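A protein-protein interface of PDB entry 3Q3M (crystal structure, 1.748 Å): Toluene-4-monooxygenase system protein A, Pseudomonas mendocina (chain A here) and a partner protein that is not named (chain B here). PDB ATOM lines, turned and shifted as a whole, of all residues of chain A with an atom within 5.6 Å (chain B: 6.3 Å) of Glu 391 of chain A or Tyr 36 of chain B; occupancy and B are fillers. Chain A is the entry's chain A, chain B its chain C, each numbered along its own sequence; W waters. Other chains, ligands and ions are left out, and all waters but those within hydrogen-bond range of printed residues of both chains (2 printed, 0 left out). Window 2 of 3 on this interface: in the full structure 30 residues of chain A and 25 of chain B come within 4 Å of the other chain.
The backbone carbonyl oxygen of Asp 386 of chain A sits at hydrogen-bond distance from the guanidinium group of Arg 41 of chain B, 3.3 Å away.
The guanidinium group (NH1) of Arg 41 of chain B is in hydrogen-bond range of the backbone carbonyl oxygen (O) of Ser 389 of chain A (2.8 Å).
The side-chain carboxylate (OE1) of Glu 391 of chain A sits at hydrogen-bond distance from the side-chain hydroxyl (OH) of Tyr 36 of chain B.
OE2 of Glu 391 of chain A is in salt-bridge range of NH2 of Arg 41 of chain B.
The backbone carbonyl oxygen (O) of Tyr 36 of chain B is in hydrogen-bond range of the guanidinium group (NE) of Arg 41 of chain B.
Among the printed residues, merely in contact across the chains: Glu 391 of chain A with His 37 of chain B (3.5 Å) and Thr 392 of chain A with His 37 of chain B (3.7 Å).
Of the printed residues of chain B, Glu 391 of chain A touches Tyr 36, His 37 and Arg 41.
Printed residues of chain A within 4 Å of Arg 41 of chain B: Asp 386, Ser 389 and Glu 391.
Of the printed residues of chain B, Ser 389 of chain A touches Arg 41 (2.8 Å).
Printed residues of chain B within 4 Å of Asp 386 of chain A: Arg 41.
Printed residues of chain B within 4 Å of Thr 392 of chain A: His 37.
Of the printed residues of chain A, His 37 of chain B touches Glu 391 and Thr 392.
Phe 10 of chain B touches none of the printed residues of chain A.
Cys 38 of chain B touches none of the printed residues of chain A.
The nearest printed residue of chain B that does not touch Glu 391 of chain A is Cys 38 of chain B (8.6 Å).
The nearest printed residue of chain B that does not touch Asp 386 of chain A is Tyr 36 of chain B (6.3 Å).
Of the 11 printed residues of chain B, 3 touch a printed residue of chain A.
Hydrophobic or aromatic side chains of chain B that line the printed part of chain A: Tyr 36 and His 37.
Water W1 bridges the side-chain carboxylate (OE2) of Glu 391 of chain A and the side-chain hydroxyl (OH) of Tyr 36 of chain B.
Water W2 lies within hydrogen-bond range of the backbone NH (N) of Glu 391 of chain A and a ring nitrogen (ND1) of His 37 of chain B.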
ATOM      1  N   ASP A 386     -15.903  -4.719 -10.256  1.00  0.00           N
ATOM      2  CA  ASP A 386     -15.105  -5.357 -11.290  1.00  0.00           C
ATOM      3  C   ASP A 386     -14.646  -4.325 -12.320  1.00  0.00           C
ATOM      4  O   ASP A 386     -13.587  -4.471 -12.919  1.00  0.00           O
ATOM      5  CB  ASP A 386     -15.849  -6.522 -11.966  1.00  0.00           C
ATOM      6  CG  ASP A 386     -17.169  -6.102 -12.572  1.00  0.00           C
ATOM      7  OD1 ASP A 386     -17.488  -6.560 -13.690  1.00  0.00           O
ATOM      8  OD2 ASP A 386     -17.895  -5.307 -11.939  1.00  0.00           O
ATOM      9  N   SER A 389     -11.308  -2.111 -11.497  1.00  0.00           N
ATOM     10  CA  SER A 389     -10.015  -2.778 -11.422  1.00  0.00           C
ATOM     11  C   SER A 389      -9.646  -3.250 -12.815  1.00  0.00           C
ATOM     12  O   SER A 389     -10.514  -3.703 -13.553  1.00  0.00           O
ATOM     13  CB  SER A 389     -10.086  -3.971 -10.492  1.00  0.00           C
ATOM     14  OG  SER A 389     -10.159  -3.512  -9.157  1.00  0.00           O
ATOM     15  N   PRO A 390      -8.357  -3.145 -13.179  1.00  0.00           N
ATOM     16  CA  PRO A 390      -7.986  -3.441 -14.568  1.00  0.00           C
ATOM     17  C   PRO A 390      -7.831  -4.932 -14.852  1.00  0.00           C
ATOM     18  O   PRO A 390      -7.561  -5.725 -13.954  1.00  0.00           O
ATOM     19  CB  PRO A 390      -6.619  -2.742 -14.714  1.00  0.00           C
ATOM     20  CG  PRO A 390      -6.024  -2.820 -13.342  1.00  0.00           C
ATOM     21  CD  PRO A 390      -7.200  -2.751 -12.358  1.00  0.00           C
ATOM     22  N   GLU A 391      -7.971  -5.285 -16.120  1.00  0.00           N
ATOM     23  CA  GLU A 391      -7.802  -6.648 -16.584  1.00  0.00           C
ATOM     24  C   GLU A 391      -6.811  -6.663 -17.748  1.00  0.00           C
ATOM     25  O   GLU A 391      -6.721  -7.640 -18.489  1.00  0.00           O
ATOM     26  CB  GLU A 391      -9.159  -7.240 -16.972  1.00  0.00           C
ATOM     27  CG  GLU A 391     -10.114  -7.242 -15.780  1.00  0.00           C
ATOM     28  CD  GLU A 391     -11.481  -7.788 -16.125  1.00  0.00           C
ATOM     29  OE1 GLU A 391     -11.582  -8.546 -17.114  1.00  0.00           O
ATOM     30  OE2 GLU A 391     -12.452  -7.432 -15.419  1.00  0.00           O
ATOM     31  N   THR A 392      -6.055  -5.577 -17.901  1.00  0.00           N
ATOM     32  CA  THR A 392      -4.915  -5.572 -18.833  1.00  0.00           C
ATOM     33  C   THR A 392      -3.824  -4.618 -18.353  1.00  0.00           C
ATOM     34  O   THR A 392      -3.982  -3.966 -17.313  1.00  0.00           O
ATOM     35  CB  THR A 392      -5.328  -5.222 -20.285  1.00  0.00           C
ATOM     36  OG1 THR A 392      -4.230  -5.511 -21.158  1.00  0.00           O
ATOM     37  CG2 THR A 392      -5.692  -3.733 -20.414  1.00  0.00           C
ATOM     38  N   LEU A 393      -2.712  -4.554 -19.091  1.00  0.00           N
ATOM     39  CA  LEU A 393      -1.609  -3.650 -18.748  1.00  0.00           C
ATOM     40  C   LEU A 393      -1.737  -2.334 -19.494  1.00  0.00           C
ATOM     41  O   LEU A 393      -2.161  -2.331 -20.655  1.00  0.00           O
ATOM     42  CB  LEU A 393      -0.244  -4.265 -19.114  1.00  0.00           C
ATOM     43  CG  LEU A 393       0.301  -5.423 -18.269  1.00  0.00           C
ATOM     44  CD1 LEU A 393       1.638  -5.879 -18.816  1.00  0.00           C
ATOM     45  CD2 LEU A 393       0.451  -5.016 -16.824  1.00  0.00           C
ATOM     46  N   PHE B  10      -8.316   4.259 -26.956  1.00  0.00           N
ATOM     47  CA  PHE B  10      -9.756   4.374 -27.191  1.00  0.00           C
ATOM     48  C   PHE B  10     -10.242   5.824 -27.047  1.00  0.00           C
ATOM     49  O   PHE B  10      -9.841   6.530 -26.132  1.00  0.00           O
ATOM     50  CB  PHE B  10     -10.521   3.492 -26.216  1.00  0.00           C
ATOM     51  CG  PHE B  10     -11.946   3.227 -26.633  1.00  0.00           C
ATOM     52  CD1 PHE B  10     -12.957   4.102 -26.280  1.00  0.00           C
ATOM     53  CD2 PHE B  10     -12.267   2.094 -27.360  1.00  0.00           C
ATOM     54  CE1 PHE B  10     -14.286   3.850 -26.672  1.00  0.00           C
ATOM     55  CE2 PHE B  10     -13.585   1.826 -27.735  1.00  0.00           C
ATOM     56  CZ  PHE B  10     -14.589   2.710 -27.406  1.00  0.00           C
ATOM     57  N   ALA B  31     -12.137  -3.801 -32.284  1.00  0.00           N
ATOM     58  CA  ALA B  31     -12.746  -2.653 -31.596  1.00  0.00           C
ATOM     59  C   ALA B  31     -13.468  -3.082 -30.308  1.00  0.00           C
ATOM     60  O   ALA B  31     -13.389  -2.405 -29.267  1.00  0.00           O
ATOM     61  CB  ALA B  31     -13.703  -1.936 -32.531  1.00  0.00           C
ATOM     62  N   GLU B  32     -14.160  -4.214 -30.380  1.00  0.00           N
ATOM     63  CA  GLU B  32     -14.902  -4.732 -29.236  1.00  0.00           C
ATOM     64  C   GLU B  32     -13.945  -5.198 -28.136  1.00  0.00           C
ATOM     65  O   GLU B  32     -14.197  -4.996 -26.953  1.00  0.00           O
ATOM     66  CB  GLU B  32     -15.843  -5.867 -29.665  1.00  0.00           C
ATOM     67  CG  GLU B  32     -16.753  -6.350 -28.556  1.00  0.00           C
ATOM     68  CD  GLU B  32     -17.418  -5.199 -27.807  1.00  0.00           C
ATOM     69  OE1 GLU B  32     -18.161  -4.424 -28.453  1.00  0.00           O
ATOM     70  OE2 GLU B  32     -17.180  -5.062 -26.576  1.00  0.00           O
ATOM     71  N   LYS B  33     -12.835  -5.817 -28.524  1.00  0.00           N
ATOM     72  CA  LYS B  33     -11.836  -6.217 -27.533  1.00  0.00           C
ATOM     73  C   LYS B  33     -11.211  -5.019 -26.814  1.00  0.00           C
ATOM     74  O   LYS B  33     -10.996  -5.070 -25.608  1.00  0.00           O
ATOM     75  CB  LYS B  33     -10.763  -7.098 -28.170  1.00  0.00           C
ATOM     76  CG  LYS B  33     -11.308  -8.488 -28.465  1.00  0.00           C
ATOM     77  CD  LYS B  33     -10.291  -9.396 -29.131  1.00  0.00           C
ATOM     78  CE  LYS B  33     -10.959 -10.753 -29.443  1.00  0.00           C
ATOM     79  NZ  LYS B  33      -9.983 -11.747 -30.003  1.00  0.00           N
ATOM     80  N   VAL B  34     -10.914  -3.953 -27.550  1.00  0.00           N
ATOM     81  CA  VAL B  34     -10.412  -2.735 -26.915  1.00  0.00           C
ATOM     82  C   VAL B  34     -11.502  -2.114 -26.038  1.00  0.00           C
ATOM     83  O   VAL B  34     -11.247  -1.746 -24.895  1.00  0.00           O
ATOM     84  CB  VAL B  34      -9.898  -1.703 -27.938  1.00  0.00           C
ATOM     85  CG1 VAL B  34      -9.431  -0.432 -27.221  1.00  0.00           C
ATOM     86  CG2 VAL B  34      -8.750  -2.306 -28.755  1.00  0.00           C
ATOM     87  N   ALA B  35     -12.726  -2.019 -26.557  1.00  0.00           N
ATOM     88  CA  ALA B  35     -13.794  -1.377 -25.781  1.00  0.00           C
ATOM     89  C   ALA B  35     -14.011  -2.034 -24.414  1.00  0.00           C
ATOM     90  O   ALA B  35     -14.374  -1.350 -23.438  1.00  0.00           O
ATOM     91  CB  ALA B  35     -15.092  -1.338 -26.573  1.00  0.00           C
ATOM     92  N   TYR B  36     -13.790  -3.347 -24.343  1.00  0.00           N
ATOM     93  CA  TYR B  36     -13.968  -4.096 -23.111  1.00  0.00           C
ATOM     94  C   TYR B  36     -13.178  -3.461 -21.982  1.00  0.00           C
ATOM     95  O   TYR B  36     -13.626  -3.451 -20.838  1.00  0.00           O
ATOM     96  CB  TYR B  36     -13.522  -5.554 -23.281  1.00  0.00           C
ATOM     97  CG  TYR B  36     -13.605  -6.352 -22.004  1.00  0.00           C
ATOM     98  CD1 TYR B  36     -14.733  -7.118 -21.706  1.00  0.00           C
ATOM     99  CD2 TYR B  36     -12.563  -6.349 -21.091  1.00  0.00           C
ATOM    100  CE1 TYR B  36     -14.812  -7.852 -20.526  1.00  0.00           C
ATOM    101  CE2 TYR B  36     -12.641  -7.074 -19.904  1.00  0.00           C
ATOM    102  CZ  TYR B  36     -13.759  -7.826 -19.635  1.00  0.00           C
ATOM    103  OH  TYR B  36     -13.839  -8.550 -18.472  1.00  0.00           O
ATOM    104  N   HIS B  37     -12.002  -2.934 -22.306  1.00  0.00           N
ATOM    105  CA  HIS B  37     -11.107  -2.385 -21.291  1.00  0.00           C
ATOM    106  C   HIS B  37     -11.267  -0.894 -21.045  1.00  0.00           C
ATOM    107  O   HIS B  37     -10.449  -0.286 -20.319  1.00  0.00           O
ATOM    108  CB  HIS B  37      -9.662  -2.700 -21.667  1.00  0.00           C
ATOM    109  CG  HIS B  37      -9.360  -4.166 -21.662  1.00  0.00           C
ATOM    110  ND1 HIS B  37      -9.207  -4.884 -20.495  1.00  0.00           N
ATOM    111  CD2 HIS B  37      -9.211  -5.052 -22.673  1.00  0.00           C
ATOM    112  CE1 HIS B  37      -8.963  -6.149 -20.789  1.00  0.00           C
ATOM    113  NE2 HIS B  37      -8.962  -6.278 -22.105  1.00  0.00           N
ATOM    114  N   CYS B  38     -12.296  -0.301 -21.652  1.00  0.00           N
ATOM    115  CA  CYS B  38     -12.445   1.163 -21.689  1.00  0.00           C
ATOM    116  C   CYS B  38     -13.865   1.641 -21.413  1.00  0.00           C
ATOM    117  O   CYS B  38     -14.096   2.432 -20.498  1.00  0.00           O
ATOM    118  CB  CYS B  38     -12.010   1.716 -23.052  1.00  0.00           C
ATOM    119  SG  CYS B  38     -10.319   1.329 -23.498  1.00  0.00           S
ATOM    120  N   VAL B  39     -14.810   1.184 -22.225  1.00  0.00           N
ATOM    121  CA  VAL B  39     -16.203   1.584 -22.082  1.00  0.00           C
ATOM    122  C   VAL B  39     -16.814   1.056 -20.775  1.00  0.00           C
ATOM    123  O   VAL B  39     -16.624  -0.106 -20.419  1.00  0.00           O
ATOM    124  CB  VAL B  39     -17.023   1.111 -23.303  1.00  0.00           C
ATOM    125  CG1 VAL B  39     -18.481   1.536 -23.189  1.00  0.00           C
ATOM    126  CG2 VAL B  39     -16.395   1.665 -24.584  1.00  0.00           C
ATOM    127  N   ARG B  41     -15.732   1.749 -18.020  1.00  0.00           N
ATOM    128  CA  ARG B  41     -14.668   1.771 -17.024  1.00  0.00           C
ATOM    129  C   ARG B  41     -14.169   3.193 -16.802  1.00  0.00           C
ATOM    130  O   ARG B  41     -14.127   3.673 -15.672  1.00  0.00           O
ATOM    131  CB  ARG B  41     -13.506   0.829 -17.401  1.00  0.00           C
ATOM    132  CG  ARG B  41     -13.909  -0.666 -17.444  1.00  0.00           C
ATOM    133  CD  ARG B  41     -12.739  -1.561 -17.876  1.00  0.00           C
ATOM    134  NE  ARG B  41     -13.132  -2.964 -17.828  1.00  0.00           N
ATOM    135  CZ  ARG B  41     -12.900  -3.762 -16.795  1.00  0.00           C
ATOM    136  NH1 ARG B  41     -12.250  -3.301 -15.744  1.00  0.00           N
ATOM    137  NH2 ARG B  41     -13.307  -5.023 -16.824  1.00  0.00           N
HETATM  138  O   HOH W   1     -14.386  -9.262 -15.104  1.00  0.00           O
HETATM  139  O   HOH W   2      -9.320  -3.593 -17.951  1.00  0.00           O
